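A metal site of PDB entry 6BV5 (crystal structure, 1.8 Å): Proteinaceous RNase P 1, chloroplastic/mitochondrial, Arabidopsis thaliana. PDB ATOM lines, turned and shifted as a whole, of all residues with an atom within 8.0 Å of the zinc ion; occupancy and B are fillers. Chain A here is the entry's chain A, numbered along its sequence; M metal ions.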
ATOM      1  N   ASN A 261      18.185  -2.274 -11.466  1.00  0.00           N
ATOM      2  CA  ASN A 261      18.655  -1.704 -12.736  1.00  0.00           C
ATOM      3  C   ASN A 261      19.551  -0.514 -12.387  1.00  0.00           C
ATOM      4  O   ASN A 261      19.083   0.492 -11.834  1.00  0.00           O
ATOM      5  CB  ASN A 261      17.485  -1.227 -13.596  1.00  0.00           C
ATOM      6  CG  ASN A 261      16.619  -2.385 -14.074  1.00  0.00           C
ATOM      7  OD1 ASN A 261      17.079  -3.533 -14.226  1.00  0.00           O
ATOM      8  ND2 ASN A 261      15.341  -2.099 -14.345  1.00  0.00           N
ATOM      9  N   LYS A 263      22.369   2.202 -13.637  1.00  0.00           N
ATOM     10  CA  LYS A 263      22.896   2.897 -14.826  1.00  0.00           C
ATOM     11  C   LYS A 263      23.648   4.136 -14.436  1.00  0.00           C
ATOM     12  O   LYS A 263      23.244   4.822 -13.500  1.00  0.00           O
ATOM     13  CB  LYS A 263      21.766   3.292 -15.771  1.00  0.00           C
ATOM     14  CG  LYS A 263      20.929   2.136 -16.295  1.00  0.00           C
ATOM     15  CD  LYS A 263      21.729   1.203 -17.199  1.00  0.00           C
ATOM     16  CE  LYS A 263      20.988  -0.096 -17.473  1.00  0.00           C
ATOM     17  NZ  LYS A 263      21.674  -0.841 -18.568  1.00  0.00           N
ATOM     18  N   THR A 265      24.405   7.893 -15.356  1.00  0.00           N
ATOM     19  CA  THR A 265      23.507   8.829 -16.020  1.00  0.00           C
ATOM     20  C   THR A 265      23.808  10.250 -15.553  1.00  0.00           C
ATOM     21  O   THR A 265      24.838  10.485 -14.923  1.00  0.00           O
ATOM     22  CB  THR A 265      22.039   8.419 -15.787  1.00  0.00           C
ATOM     23  OG1 THR A 265      21.196   9.176 -16.635  1.00  0.00           O
ATOM     24  CG2 THR A 265      21.617   8.605 -14.337  1.00  0.00           C
ATOM     25  N   GLU A 266      22.953  11.186 -15.936  1.00  0.00           N
ATOM     26  CA  GLU A 266      23.097  12.589 -15.587  1.00  0.00           C
ATOM     27  C   GLU A 266      21.749  13.106 -15.197  1.00  0.00           C
ATOM     28  O   GLU A 266      20.713  12.482 -15.479  1.00  0.00           O
ATOM     29  CB  GLU A 266      23.597  13.371 -16.786  1.00  0.00           C
ATOM     30  CG  GLU A 266      24.993  12.995 -17.241  1.00  0.00           C
ATOM     31  CD  GLU A 266      25.351  13.586 -18.604  1.00  0.00           C
ATOM     32  OE1 GLU A 266      24.467  14.159 -19.286  1.00  0.00           O
ATOM     33  OE2 GLU A 266      26.538  13.485 -18.979  1.00  0.00           O
ATOM     34  N   MET A 267      21.763  14.267 -14.532  1.00  0.00           N
ATOM     35  CA  MET A 267      20.577  14.993 -14.193  1.00  0.00           C
ATOM     36  C   MET A 267      20.502  16.126 -15.193  1.00  0.00           C
ATOM     37  O   MET A 267      21.531  16.659 -15.588  1.00  0.00           O
ATOM     38  CB  MET A 267      20.679  15.545 -12.770  1.00  0.00           C
ATOM     39  CG  MET A 267      20.858  14.461 -11.720  1.00  0.00           C
ATOM     40  SD  MET A 267      19.415  13.403 -11.621  1.00  0.00           S
ATOM     41  CE  MET A 267      20.216  11.804 -11.671  1.00  0.00           C
ATOM     42  N   VAL A 272      16.137  16.393 -12.952  1.00  0.00           N
ATOM     43  CA  VAL A 272      15.388  15.226 -13.403  1.00  0.00           C
ATOM     44  C   VAL A 272      16.381  14.189 -13.933  1.00  0.00           C
ATOM     45  O   VAL A 272      17.198  14.489 -14.803  1.00  0.00           O
ATOM     46  CB  VAL A 272      14.346  15.580 -14.494  1.00  0.00           C
ATOM     47  CG1 VAL A 272      13.705  14.319 -15.061  1.00  0.00           C
ATOM     48  CG2 VAL A 272      13.276  16.507 -13.927  1.00  0.00           C
ATOM     49  N   CYS A 273      16.295  12.957 -13.385  1.00  0.00           N
ATOM     50  CA  CYS A 273      17.159  11.849 -13.826  1.00  0.00           C
ATOM     51  C   CYS A 273      16.813  11.483 -15.273  1.00  0.00           C
ATOM     52  O   CYS A 273      15.650  11.242 -15.576  1.00  0.00           O
ATOM     53  CB  CYS A 273      16.984  10.607 -12.925  1.00  0.00           C
ATOM     54  SG  CYS A 273      17.978   9.159 -13.431  1.00  0.00           S
ATOM     55  N   LYS A 274      17.812  11.459 -16.133  1.00  0.00           N
ATOM     56  CA  LYS A 274      17.630  11.094 -17.532  1.00  0.00           C
ATOM     57  C   LYS A 274      17.320   9.598 -17.745  1.00  0.00           C
ATOM     58  O   LYS A 274      16.710   9.243 -18.746  1.00  0.00           O
ATOM     59  CB  LYS A 274      18.854  11.486 -18.360  1.00  0.00           C
ATOM     60  CG  LYS A 274      18.998  12.986 -18.509  1.00  0.00           C
ATOM     61  CD  LYS A 274      20.249  13.362 -19.303  1.00  0.00           C
ATOM     62  CE  LYS A 274      20.375  14.880 -19.442  1.00  0.00           C
ATOM     63  NZ  LYS A 274      21.771  15.241 -19.779  1.00  0.00           N
ATOM     64  N   CYS A 275      17.714   8.743 -16.800  1.00  0.00           N
ATOM     65  CA  CYS A 275      17.396   7.320 -16.862  1.00  0.00           C
ATOM     66  C   CYS A 275      15.959   7.026 -16.414  1.00  0.00           C
ATOM     67  O   CYS A 275      15.213   6.426 -17.175  1.00  0.00           O
ATOM     68  CB  CYS A 275      18.397   6.515 -16.051  1.00  0.00           C
ATOM     69  SG  CYS A 275      18.104   4.733 -16.140  1.00  0.00           S
ATOM     70  N   CYS A 276      15.547   7.463 -15.220  1.00  0.00           N
ATOM     71  CA  CYS A 276      14.222   7.103 -14.678  1.00  0.00           C
ATOM     72  C   CYS A 276      13.188   8.236 -14.606  1.00  0.00           C
ATOM     73  O   CYS A 276      12.047   7.982 -14.210  1.00  0.00           O
ATOM     74  CB  CYS A 276      14.371   6.500 -13.280  1.00  0.00           C
ATOM     75  SG  CYS A 276      14.816   7.669 -11.951  1.00  0.00           S
ATOM     76  N   LYS A 277      13.579   9.483 -14.917  1.00  0.00           N
ATOM     77  CA  LYS A 277      12.672  10.656 -14.851  1.00  0.00           C
ATOM     78  C   LYS A 277      12.209  11.062 -13.438  1.00  0.00           C
ATOM     79  O   LYS A 277      11.268  11.860 -13.304  1.00  0.00           O
ATOM     80  CB  LYS A 277      11.450  10.478 -15.779  1.00  0.00           C
ATOM     81  CG  LYS A 277      11.781  10.022 -17.196  1.00  0.00           C
ATOM     82  CD  LYS A 277      12.663  11.020 -17.941  1.00  0.00           C
ATOM     83  CE  LYS A 277      12.945  10.587 -19.367  1.00  0.00           C
ATOM     84  NZ  LYS A 277      14.069   9.607 -19.442  1.00  0.00           N
ATOM     85  N   GLU A 278      12.852  10.550 -12.391  1.00  0.00           N
ATOM     86  CA  GLU A 278      12.616  11.010 -11.023  1.00  0.00           C
ATOM     87  C   GLU A 278      13.129  12.470 -10.901  1.00  0.00           C
ATOM     88  O   GLU A 278      14.220  12.751 -11.352  1.00  0.00           O
ATOM     89  CB  GLU A 278      13.394  10.141 -10.056  1.00  0.00           C
ATOM     90  CG  GLU A 278      13.367  10.563  -8.573  1.00  0.00           C
ATOM     91  CD  GLU A 278      12.625   9.600  -7.677  1.00  0.00           C
ATOM     92  OE1 GLU A 278      12.637   8.379  -7.954  1.00  0.00           O
ATOM     93  OE2 GLU A 278      12.054  10.081  -6.672  1.00  0.00           O
ATOM     94  N   LYS A 279      12.349  13.352 -10.290  1.00  0.00           N
ATOM     95  CA  LYS A 279      12.831  14.705  -9.988  1.00  0.00           C
ATOM     96  C   LYS A 279      13.492  14.696  -8.607  1.00  0.00           C
ATOM     97  O   LYS A 279      12.842  14.446  -7.603  1.00  0.00           O
ATOM     98  CB  LYS A 279      11.709  15.734 -10.066  1.00  0.00           C
ATOM     99  CG  LYS A 279      12.229  17.180 -10.090  1.00  0.00           C
ATOM    100  CD  LYS A 279      11.106  18.187 -10.290  1.00  0.00           C
ATOM    101  CE  LYS A 279      11.428  19.550  -9.695  1.00  0.00           C
ATOM    102  NZ  LYS A 279      12.475  20.285 -10.450  1.00  0.00           N
ATOM    103  N   LEU A 280      14.785  14.974  -8.566  1.00  0.00           N
ATOM    104  CA  LEU A 280      15.500  15.044  -7.296  1.00  0.00           C
ATOM    105  C   LEU A 280      14.983  16.204  -6.455  1.00  0.00           C
ATOM    106  O   LEU A 280      14.428  17.165  -6.981  1.00  0.00           O
ATOM    107  CB  LEU A 280      17.003  15.171  -7.541  1.00  0.00           C
ATOM    108  CG  LEU A 280      17.708  13.993  -8.194  1.00  0.00           C
ATOM    109  CD1 LEU A 280      19.211  14.145  -8.068  1.00  0.00           C
ATOM    110  CD2 LEU A 280      17.268  12.681  -7.568  1.00  0.00           C
ATOM    111  N   THR A 475      14.360   4.121  -4.520  1.00  0.00           N
ATOM    112  CA  THR A 475      15.277   4.414  -5.628  1.00  0.00           C
ATOM    113  C   THR A 475      16.416   5.283  -5.122  1.00  0.00           C
ATOM    114  O   THR A 475      16.195   6.205  -4.334  1.00  0.00           O
ATOM    115  CB  THR A 475      14.507   5.108  -6.771  1.00  0.00           C
ATOM    116  OG1 THR A 475      13.440   4.246  -7.171  1.00  0.00           O
ATOM    117  CG2 THR A 475      15.397   5.377  -7.988  1.00  0.00           C
ATOM    118  N   TRP A 476      17.627   4.972  -5.574  1.00  0.00           N
ATOM    119  CA  TRP A 476      18.810   5.696  -5.168  1.00  0.00           C
ATOM    120  C   TRP A 476      19.399   6.483  -6.320  1.00  0.00           C
ATOM    121  O   TRP A 476      19.521   5.957  -7.425  1.00  0.00           O
ATOM    122  CB  TRP A 476      19.865   4.744  -4.614  1.00  0.00           C
ATOM    123  CG  TRP A 476      19.505   4.186  -3.293  1.00  0.00           C
ATOM    124  CD1 TRP A 476      18.675   3.130  -3.044  1.00  0.00           C
ATOM    125  CD2 TRP A 476      19.964   4.645  -2.030  1.00  0.00           C
ATOM    126  NE1 TRP A 476      18.588   2.910  -1.699  1.00  0.00           N
ATOM    127  CE2 TRP A 476      19.374   3.823  -1.051  1.00  0.00           C
ATOM    128  CE3 TRP A 476      20.834   5.670  -1.613  1.00  0.00           C
ATOM    129  CZ2 TRP A 476      19.611   4.001   0.317  1.00  0.00           C
ATOM    130  CZ3 TRP A 476      21.073   5.846  -0.254  1.00  0.00           C
ATOM    131  CH2 TRP A 476      20.455   5.013   0.697  1.00  0.00           C
ATOM    132  N   HIS A 477      19.782   7.739  -6.055  1.00  0.00           N
ATOM    133  CA  HIS A 477      20.612   8.522  -6.973  1.00  0.00           C
ATOM    134  C   HIS A 477      21.889   8.958  -6.258  1.00  0.00           C
ATOM    135  O   HIS A 477      21.830   9.580  -5.192  1.00  0.00           O
ATOM    136  CB  HIS A 477      19.824   9.674  -7.533  1.00  0.00           C
ATOM    137  CG  HIS A 477      18.707   9.237  -8.416  1.00  0.00           C
ATOM    138  ND1 HIS A 477      17.449   8.985  -7.925  1.00  0.00           N
ATOM    139  CD2 HIS A 477      18.662   8.956  -9.732  1.00  0.00           C
ATOM    140  CE1 HIS A 477      16.665   8.580  -8.911  1.00  0.00           C
ATOM    141  NE2 HIS A 477      17.382   8.546 -10.013  1.00  0.00           N
ATOM    142  N   VAL A 478      23.032   8.608  -6.828  1.00  0.00           N
ATOM    143  CA  VAL A 478      24.327   8.809  -6.174  1.00  0.00           C
ATOM    144  C   VAL A 478      25.186   9.693  -7.090  1.00  0.00           C
ATOM    145  O   VAL A 478      25.508   9.291  -8.201  1.00  0.00           O
ATOM    146  CB  VAL A 478      25.023   7.463  -5.871  1.00  0.00           C
ATOM    147  CG1 VAL A 478      26.429   7.684  -5.340  1.00  0.00           C
ATOM    148  CG2 VAL A 478      24.158   6.670  -4.884  1.00  0.00           C
ATOM    149  N   TRP A 492      26.069  10.458 -12.378  1.00  0.00           N
ATOM    150  CA  TRP A 492      25.276   9.934 -11.312  1.00  0.00           C
ATOM    151  C   TRP A 492      25.045   8.456 -11.517  1.00  0.00           C
ATOM    152  O   TRP A 492      25.011   7.964 -12.645  1.00  0.00           O
ATOM    153  CB  TRP A 492      23.932  10.610 -11.287  1.00  0.00           C
ATOM    154  CG  TRP A 492      23.917  12.031 -10.849  1.00  0.00           C
ATOM    155  CD1 TRP A 492      24.349  13.124 -11.570  1.00  0.00           C
ATOM    156  CD2 TRP A 492      23.391  12.542  -9.623  1.00  0.00           C
ATOM    157  NE1 TRP A 492      24.117  14.279 -10.846  1.00  0.00           N
ATOM    158  CE2 TRP A 492      23.540  13.958  -9.663  1.00  0.00           C
ATOM    159  CE3 TRP A 492      22.849  11.938  -8.483  1.00  0.00           C
ATOM    160  CZ2 TRP A 492      23.137  14.769  -8.608  1.00  0.00           C
ATOM    161  CZ3 TRP A 492      22.434  12.762  -7.436  1.00  0.00           C
ATOM    162  CH2 TRP A 492      22.580  14.169  -7.517  1.00  0.00           C
ATOM    163  N   LEU A 493      24.822   7.750 -10.407  1.00  0.00           N
ATOM    164  CA  LEU A 493      24.282   6.387 -10.465  1.00  0.00           C
ATOM    165  C   LEU A 493      22.785   6.457 -10.216  1.00  0.00           C
ATOM    166  O   LEU A 493      22.346   7.108  -9.260  1.00  0.00           O
ATOM    167  CB  LEU A 493      24.969   5.508  -9.415  1.00  0.00           C
ATOM    168  CG  LEU A 493      25.034   4.014  -9.722  1.00  0.00           C
ATOM    169  CD1 LEU A 493      25.865   3.780 -10.984  1.00  0.00           C
ATOM    170  CD2 LEU A 493      25.625   3.273  -8.522  1.00  0.00           C
ATOM    171  N   CYS A 494      22.006   5.795 -11.090  1.00  0.00           N
ATOM    172  CA  CYS A 494      20.573   5.596 -10.881  1.00  0.00           C
ATOM    173  C   CYS A 494      20.403   4.101 -10.568  1.00  0.00           C
ATOM    174  O   CYS A 494      20.675   3.273 -11.431  1.00  0.00           O
ATOM    175  CB  CYS A 494      19.781   5.939 -12.121  1.00  0.00           C
ATOM    176  SG  CYS A 494      17.999   5.620 -12.026  1.00  0.00           S
ATOM    177  N   ALA A 495      19.991   3.778  -9.346  1.00  0.00           N
ATOM    178  CA  ALA A 495      19.694   2.398  -8.929  1.00  0.00           C
ATOM    179  C   ALA A 495      18.216   2.283  -8.594  1.00  0.00           C
ATOM    180  O   ALA A 495      17.738   2.842  -7.604  1.00  0.00           O
ATOM    181  CB  ALA A 495      20.559   1.993  -7.737  1.00  0.00           C
ATOM    182  N   LYS A 496      17.493   1.560  -9.435  1.00  0.00           N
ATOM    183  CA  LYS A 496      16.042   1.445  -9.361  1.00  0.00           C
ATOM    184  C   LYS A 496      15.663  -0.041  -9.490  1.00  0.00           C
ATOM    185  O   LYS A 496      16.238  -0.724 -10.333  1.00  0.00           O
ATOM    186  CB  LYS A 496      15.428   2.223 -10.534  1.00  0.00           C
ATOM    187  CG  LYS A 496      13.925   2.395 -10.466  1.00  0.00           C
ATOM    188  CD  LYS A 496      13.479   3.510 -11.409  1.00  0.00           C
ATOM    189  CE  LYS A 496      11.969   3.598 -11.568  1.00  0.00           C
ATOM    190  NZ  LYS A 496      11.299   3.908 -10.277  1.00  0.00           N
HETATM  191 ZN    ZN M   1      16.997   7.703 -11.874  1.00  0.00          ZN
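The side-chain sulfur of Cys 273 sits close to the backbone NH of Cys 275, at 3.4 Å. N of Cys 494 sits at hydrogen-bond distance from O of Lys 263, 2.9 Å away. The backbone NH (N) of Cys 273 sits close to the side-chain sulfur (SD) of Met 267, 3.6 Å away. The backbone NH (N) of Cys 273 sits at hydrogen-bond distance from the backbone carbonyl oxygen (O) of Glu 278 (2.9 Å). The side-chain sulfur (SG) of Cys 276 lies close to the backbone NH (N) of Glu 278 (3.5 Å).
The zinc ion is bound by a ring nitrogen (NE2) of His 477, the side-chain sulfur (SG) of Cys 276, the side-chain sulfur (SG) of Cys 494 and the side-chain sulfur (SG) of Cys 273.
Four residues have an atom within 4 Å of the zinc ion: Cys 273, Cys 276, His 477 and Cys 494.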
